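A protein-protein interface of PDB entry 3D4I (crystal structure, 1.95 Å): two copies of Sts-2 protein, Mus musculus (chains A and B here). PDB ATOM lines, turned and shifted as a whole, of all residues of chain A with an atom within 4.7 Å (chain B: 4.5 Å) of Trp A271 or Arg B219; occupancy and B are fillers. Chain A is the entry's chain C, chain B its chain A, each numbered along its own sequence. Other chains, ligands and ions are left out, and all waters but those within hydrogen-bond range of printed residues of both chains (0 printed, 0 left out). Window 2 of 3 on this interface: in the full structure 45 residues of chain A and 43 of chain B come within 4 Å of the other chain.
The guanidinium group (NH2) of Arg B219 sits at hydrogen-bond distance from the backbone carbonyl oxygen (O) of Trp A271, at 3.1 Å.
The guanidinium group of Arg B219 lies within salt-bridge range of the side-chain carboxylate of Asp B207 (2.8 Å). The backbone carbonyl oxygen (O) of Leu B206 sits at hydrogen-bond distance from the side-chain sulfur (SG) of Cys B237, 3.7 Å away. OH of Tyr B172 lies within hydrogen-bond range of O of Arg B219 (2.5 Å).
Trp A268 touches Leu B250 (CZ3 to CB, 3.7 Å). O of Leu B206 touches CH2 of Trp A271, 3.98 Å away. CD1 of Trp A271 touches CG of Leu B227 (3.5 Å). Trp A271 touches Cys B237.
Of the printed residues of chain B, Trp A271 touches Leu B206 (3.98 Å), Arg B219 (3.1 Å), Leu B227 (3.5 Å) and Cys B237 (3.1 Å). Printed residues of chain A within 4 Å of Arg B219: Trp A271 (3.1 Å). Of the printed residues of chain A, Leu B206 touches Trp A271 (3.98 Å). Of the printed residues of chain A, Cys B237 touches Trp A271 (3.1 Å). Of the printed residues of chain A, Leu B250 touches Trp A268 (3.7 Å). Arg A269 touches none of the printed residues of chain B. The nearest printed residue of chain B that does not touch Trp A271 is Leu B250 (4.3 Å). The nearest printed residue of chain A that does not touch Arg B219 is Asn A270 (6.2 Å).
Among the printed residues, no Asp or Glu carboxylate lies within 4 Å of a Lys or Arg side-chain nitrogen of the other chain.
No position is printed for both chains.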
ATOM      1  N   PHE A 266     -15.067 -23.074 -30.003  1.00  0.00           N
ATOM      2  CA  PHE A 266     -14.807 -22.155 -28.907  1.00  0.00           C
ATOM      3  C   PHE A 266     -15.796 -20.996 -28.960  1.00  0.00           C
ATOM      4  O   PHE A 266     -15.875 -20.300 -29.963  1.00  0.00           O
ATOM      5  CB  PHE A 266     -13.370 -21.656 -29.024  1.00  0.00           C
ATOM      6  CG  PHE A 266     -12.985 -20.634 -27.991  1.00  0.00           C
ATOM      7  CD1 PHE A 266     -13.060 -20.929 -26.627  1.00  0.00           C
ATOM      8  CD2 PHE A 266     -12.525 -19.379 -28.385  1.00  0.00           C
ATOM      9  CE1 PHE A 266     -12.696 -19.986 -25.676  1.00  0.00           C
ATOM     10  CE2 PHE A 266     -12.155 -18.420 -27.433  1.00  0.00           C
ATOM     11  CZ  PHE A 266     -12.237 -18.721 -26.086  1.00  0.00           C
ATOM     12  N   TRP A 268     -16.440 -17.620 -27.057  1.00  0.00           N
ATOM     13  CA  TRP A 268     -15.900 -16.633 -26.129  1.00  0.00           C
ATOM     14  C   TRP A 268     -16.888 -16.276 -25.007  1.00  0.00           C
ATOM     15  O   TRP A 268     -16.492 -16.155 -23.848  1.00  0.00           O
ATOM     16  CB  TRP A 268     -15.435 -15.374 -26.886  1.00  0.00           C
ATOM     17  CG  TRP A 268     -16.532 -14.581 -27.550  1.00  0.00           C
ATOM     18  CD1 TRP A 268     -17.060 -14.786 -28.800  1.00  0.00           C
ATOM     19  CD2 TRP A 268     -17.238 -13.462 -26.999  1.00  0.00           C
ATOM     20  NE1 TRP A 268     -18.051 -13.863 -29.056  1.00  0.00           N
ATOM     21  CE2 TRP A 268     -18.175 -13.037 -27.967  1.00  0.00           C
ATOM     22  CE3 TRP A 268     -17.173 -12.778 -25.774  1.00  0.00           C
ATOM     23  CZ2 TRP A 268     -19.033 -11.955 -27.750  1.00  0.00           C
ATOM     24  CZ3 TRP A 268     -18.026 -11.702 -25.564  1.00  0.00           C
ATOM     25  CH2 TRP A 268     -18.944 -11.302 -26.545  1.00  0.00           C
ATOM     26  N   ARG A 269     -18.168 -16.155 -25.364  1.00  0.00           N
ATOM     27  CA  ARG A 269     -19.239 -15.788 -24.430  1.00  0.00           C
ATOM     28  C   ARG A 269     -19.367 -16.704 -23.218  1.00  0.00           C
ATOM     29  O   ARG A 269     -19.928 -16.302 -22.202  1.00  0.00           O
ATOM     30  CB  ARG A 269     -20.590 -15.712 -25.148  1.00  0.00           C
ATOM     31  CG  ARG A 269     -20.842 -14.395 -25.829  1.00  0.00           C
ATOM     32  CD  ARG A 269     -22.310 -14.218 -26.159  1.00  0.00           C
ATOM     33  NE  ARG A 269     -22.573 -12.892 -26.711  1.00  0.00           N
ATOM     34  CZ  ARG A 269     -22.419 -12.568 -27.992  1.00  0.00           C
ATOM     35  NH1 ARG A 269     -21.995 -13.480 -28.862  1.00  0.00           N
ATOM     36  NH2 ARG A 269     -22.681 -11.333 -28.407  1.00  0.00           N
ATOM     37  N   ASN A 270     -18.850 -17.925 -23.326  1.00  0.00           N
ATOM     38  CA  ASN A 270     -18.831 -18.858 -22.193  1.00  0.00           C
ATOM     39  C   ASN A 270     -17.856 -18.486 -21.055  1.00  0.00           C
ATOM     40  O   ASN A 270     -17.557 -19.303 -20.175  1.00  0.00           O
ATOM     41  CB  ASN A 270     -18.673 -20.300 -22.683  1.00  0.00           C
ATOM     42  CG  ASN A 270     -19.908 -20.791 -23.426  1.00  0.00           C
ATOM     43  OD1 ASN A 270     -20.812 -20.005 -23.733  1.00  0.00           O
ATOM     44  ND2 ASN A 270     -19.951 -22.093 -23.727  1.00  0.00           N
ATOM     45  N   TRP A 271     -17.375 -17.243 -21.111  1.00  0.00           N
ATOM     46  CA  TRP A 271     -16.878 -16.483 -19.953  1.00  0.00           C
ATOM     47  C   TRP A 271     -16.980 -14.978 -20.239  1.00  0.00           C
ATOM     48  O   TRP A 271     -16.381 -14.143 -19.548  1.00  0.00           O
ATOM     49  CB  TRP A 271     -15.448 -16.874 -19.556  1.00  0.00           C
ATOM     50  CG  TRP A 271     -14.489 -17.000 -20.693  1.00  0.00           C
ATOM     51  CD1 TRP A 271     -13.947 -18.157 -21.183  1.00  0.00           C
ATOM     52  CD2 TRP A 271     -13.945 -15.937 -21.487  1.00  0.00           C
ATOM     53  NE1 TRP A 271     -13.101 -17.881 -22.228  1.00  0.00           N
ATOM     54  CE2 TRP A 271     -13.082 -16.527 -22.437  1.00  0.00           C
ATOM     55  CE3 TRP A 271     -14.103 -14.543 -21.488  1.00  0.00           C
ATOM     56  CZ2 TRP A 271     -12.387 -15.776 -23.379  1.00  0.00           C
ATOM     57  CZ3 TRP A 271     -13.411 -13.800 -22.420  1.00  0.00           C
ATOM     58  CH2 TRP A 271     -12.564 -14.420 -23.357  1.00  0.00           C
ATOM     59  N   TYR B 172       0.064 -15.956  -8.404  1.00  0.00           N
ATOM     60  CA  TYR B 172      -1.067 -15.598  -9.258  1.00  0.00           C
ATOM     61  C   TYR B 172      -1.371 -14.106  -9.163  1.00  0.00           C
ATOM     62  O   TYR B 172      -1.525 -13.442 -10.193  1.00  0.00           O
ATOM     63  CB  TYR B 172      -2.306 -16.444  -8.941  1.00  0.00           C
ATOM     64  CG  TYR B 172      -3.547 -16.029  -9.699  1.00  0.00           C
ATOM     65  CD1 TYR B 172      -3.671 -16.276 -11.070  1.00  0.00           C
ATOM     66  CD2 TYR B 172      -4.600 -15.386  -9.046  1.00  0.00           C
ATOM     67  CE1 TYR B 172      -4.818 -15.884 -11.771  1.00  0.00           C
ATOM     68  CE2 TYR B 172      -5.749 -14.985  -9.748  1.00  0.00           C
ATOM     69  CZ  TYR B 172      -5.850 -15.239 -11.093  1.00  0.00           C
ATOM     70  OH  TYR B 172      -6.987 -14.854 -11.763  1.00  0.00           O
ATOM     71  N   LEU B 206      -6.051 -14.449 -22.518  1.00  0.00           N
ATOM     72  CA  LEU B 206      -7.413 -14.114 -22.947  1.00  0.00           C
ATOM     73  C   LEU B 206      -8.249 -13.637 -21.756  1.00  0.00           C
ATOM     74  O   LEU B 206      -9.184 -12.864 -21.940  1.00  0.00           O
ATOM     75  CB  LEU B 206      -8.117 -15.247 -23.705  1.00  0.00           C
ATOM     76  CG  LEU B 206      -7.854 -15.301 -25.227  1.00  0.00           C
ATOM     77  CD1 LEU B 206      -6.509 -15.926 -25.504  1.00  0.00           C
ATOM     78  CD2 LEU B 206      -8.940 -16.077 -25.950  1.00  0.00           C
ATOM     79  N   ASP B 207      -7.875 -14.079 -20.556  1.00  0.00           N
ATOM     80  CA  ASP B 207      -8.486 -13.601 -19.312  1.00  0.00           C
ATOM     81  C   ASP B 207      -7.690 -12.434 -18.689  1.00  0.00           C
ATOM     82  O   ASP B 207      -8.233 -11.347 -18.426  1.00  0.00           O
ATOM     83  CB  ASP B 207      -8.641 -14.749 -18.297  1.00  0.00           C
ATOM     84  CG  ASP B 207      -9.519 -14.361 -17.102  1.00  0.00           C
ATOM     85  OD1 ASP B 207     -10.702 -14.028 -17.324  1.00  0.00           O
ATOM     86  OD2 ASP B 207      -9.059 -14.417 -15.943  1.00  0.00           O
ATOM     87  N   ARG B 211      -9.599  -8.653 -18.602  1.00  0.00           N
ATOM     88  CA  ARG B 211     -10.232  -8.234 -17.333  1.00  0.00           C
ATOM     89  C   ARG B 211      -9.833  -6.817 -16.866  1.00  0.00           C
ATOM     90  O   ARG B 211     -10.719  -6.032 -16.514  1.00  0.00           O
ATOM     91  CB  ARG B 211     -10.033  -9.279 -16.238  1.00  0.00           C
ATOM     92  CG  ARG B 211     -10.872 -10.527 -16.490  1.00  0.00           C
ATOM     93  CD  ARG B 211     -10.839 -11.487 -15.344  1.00  0.00           C
ATOM     94  NE  ARG B 211     -11.706 -11.073 -14.246  1.00  0.00           N
ATOM     95  CZ  ARG B 211     -13.017 -11.306 -14.169  1.00  0.00           C
ATOM     96  NH1 ARG B 211     -13.665 -11.951 -15.132  1.00  0.00           N
ATOM     97  NH2 ARG B 211     -13.683 -10.906 -13.097  1.00  0.00           N
ATOM     98  N   PRO B 217     -12.278  -7.343 -11.472  1.00  0.00           N
ATOM     99  CA  PRO B 217     -11.216  -7.847 -10.617  1.00  0.00           C
ATOM    100  C   PRO B 217     -10.706  -9.205 -11.157  1.00  0.00           C
ATOM    101  O   PRO B 217     -11.399  -9.850 -11.940  1.00  0.00           O
ATOM    102  CB  PRO B 217     -11.918  -8.011  -9.267  1.00  0.00           C
ATOM    103  CG  PRO B 217     -13.322  -8.347  -9.628  1.00  0.00           C
ATOM    104  CD  PRO B 217     -13.604  -7.517 -10.864  1.00  0.00           C
ATOM    105  N   PRO B 218      -9.491  -9.617 -10.772  1.00  0.00           N
ATOM    106  CA  PRO B 218      -9.009 -10.932 -11.201  1.00  0.00           C
ATOM    107  C   PRO B 218      -9.979 -12.030 -10.787  1.00  0.00           C
ATOM    108  O   PRO B 218     -10.594 -11.937  -9.720  1.00  0.00           O
ATOM    109  CB  PRO B 218      -7.683 -11.062 -10.443  1.00  0.00           C
ATOM    110  CG  PRO B 218      -7.212  -9.625 -10.311  1.00  0.00           C
ATOM    111  CD  PRO B 218      -8.481  -8.905  -9.960  1.00  0.00           C
ATOM    112  N   ARG B 219     -10.146 -13.038 -11.641  1.00  0.00           N
ATOM    113  CA  ARG B 219     -10.901 -14.235 -11.288  1.00  0.00           C
ATOM    114  C   ARG B 219     -10.125 -14.948 -10.201  1.00  0.00           C
ATOM    115  O   ARG B 219      -8.909 -14.811 -10.132  1.00  0.00           O
ATOM    116  CB  ARG B 219     -11.005 -15.180 -12.486  1.00  0.00           C
ATOM    117  CG  ARG B 219     -11.869 -14.699 -13.591  1.00  0.00           C
ATOM    118  CD  ARG B 219     -12.019 -15.761 -14.645  1.00  0.00           C
ATOM    119  NE  ARG B 219     -12.733 -15.234 -15.804  1.00  0.00           N
ATOM    120  CZ  ARG B 219     -14.046 -15.317 -15.983  1.00  0.00           C
ATOM    121  NH1 ARG B 219     -14.815 -15.895 -15.072  1.00  0.00           N
ATOM    122  NH2 ARG B 219     -14.591 -14.812 -17.080  1.00  0.00           N
ATOM    123  N   GLU B 220     -10.823 -15.701  -9.348  1.00  0.00           N
ATOM    124  CA  GLU B 220     -10.171 -16.618  -8.418  1.00  0.00           C
ATOM    125  C   GLU B 220      -9.267 -17.557  -9.235  1.00  0.00           C
ATOM    126  O   GLU B 220      -9.627 -17.965 -10.333  1.00  0.00           O
ATOM    127  CB  GLU B 220     -11.221 -17.425  -7.647  1.00  0.00           C
ATOM    128  CG  GLU B 220     -10.713 -18.125  -6.381  1.00  0.00           C
ATOM    129  CD  GLU B 220     -10.199 -19.555  -6.627  1.00  0.00           C
ATOM    130  OE1 GLU B 220     -10.792 -20.281  -7.461  1.00  0.00           O
ATOM    131  OE2 GLU B 220      -9.206 -19.959  -5.970  1.00  0.00           O
ATOM    132  N   CYS B 221      -8.098 -17.880  -8.687  1.00  0.00           N
ATOM    133  CA  CYS B 221      -7.081 -18.637  -9.420  1.00  0.00           C
ATOM    134  C   CYS B 221      -7.588 -19.940 -10.022  1.00  0.00           C
ATOM    135  O   CYS B 221      -7.250 -20.256 -11.161  1.00  0.00           O
ATOM    136  CB  CYS B 221      -5.883 -18.925  -8.521  1.00  0.00           C
ATOM    137  SG  CYS B 221      -4.547 -19.774  -9.377  1.00  0.00           S
ATOM    138  N   PHE B 224      -9.812 -19.261 -12.894  1.00  0.00           N
ATOM    139  CA  PHE B 224      -8.946 -18.839 -14.018  1.00  0.00           C
ATOM    140  C   PHE B 224      -8.335 -20.087 -14.697  1.00  0.00           C
ATOM    141  O   PHE B 224      -8.460 -20.267 -15.901  1.00  0.00           O
ATOM    142  CB  PHE B 224      -7.901 -17.866 -13.472  1.00  0.00           C
ATOM    143  CG  PHE B 224      -6.702 -17.627 -14.365  1.00  0.00           C
ATOM    144  CD1 PHE B 224      -6.767 -16.724 -15.423  1.00  0.00           C
ATOM    145  CD2 PHE B 224      -5.478 -18.232 -14.075  1.00  0.00           C
ATOM    146  CE1 PHE B 224      -5.634 -16.487 -16.231  1.00  0.00           C
ATOM    147  CE2 PHE B 224      -4.340 -17.989 -14.872  1.00  0.00           C
ATOM    148  CZ  PHE B 224      -4.433 -17.114 -15.944  1.00  0.00           C
ATOM    149  N   LEU B 227     -10.786 -22.042 -16.721  1.00  0.00           N
ATOM    150  CA  LEU B 227     -11.206 -21.267 -17.882  1.00  0.00           C
ATOM    151  C   LEU B 227     -10.200 -21.343 -19.015  1.00  0.00           C
ATOM    152  O   LEU B 227     -10.578 -21.514 -20.174  1.00  0.00           O
ATOM    153  CB  LEU B 227     -11.386 -19.792 -17.475  1.00  0.00           C
ATOM    154  CG  LEU B 227     -12.468 -18.888 -18.069  1.00  0.00           C
ATOM    155  CD1 LEU B 227     -13.647 -18.804 -17.114  1.00  0.00           C
ATOM    156  CD2 LEU B 227     -11.898 -17.479 -18.292  1.00  0.00           C
ATOM    157  N   CYS B 237     -10.235 -13.335 -27.915  1.00  0.00           N
ATOM    158  CA  CYS B 237     -11.096 -12.503 -27.053  1.00  0.00           C
ATOM    159  C   CYS B 237     -10.929 -11.090 -27.593  1.00  0.00           C
ATOM    160  O   CYS B 237      -9.800 -10.638 -27.732  1.00  0.00           O
ATOM    161  CB  CYS B 237     -10.570 -12.509 -25.601  1.00  0.00           C
ATOM    162  SG  CYS B 237     -11.619 -11.627 -24.447  1.00  0.00           S
ATOM    163  N   LEU B 250     -16.449  -6.260 -24.035  1.00  0.00           N
ATOM    164  CA  LEU B 250     -16.282  -7.477 -24.822  1.00  0.00           C
ATOM    165  C   LEU B 250     -17.220  -7.531 -26.029  1.00  0.00           C
ATOM    166  O   LEU B 250     -18.437  -7.305 -25.918  1.00  0.00           O
ATOM    167  CB  LEU B 250     -16.578  -8.680 -23.965  1.00  0.00           C
ATOM    168  CG  LEU B 250     -15.489  -9.293 -23.117  1.00  0.00           C
ATOM    169  CD1 LEU B 250     -16.155 -10.291 -22.226  1.00  0.00           C
ATOM    170  CD2 LEU B 250     -14.472  -9.969 -24.034  1.00  0.00           C
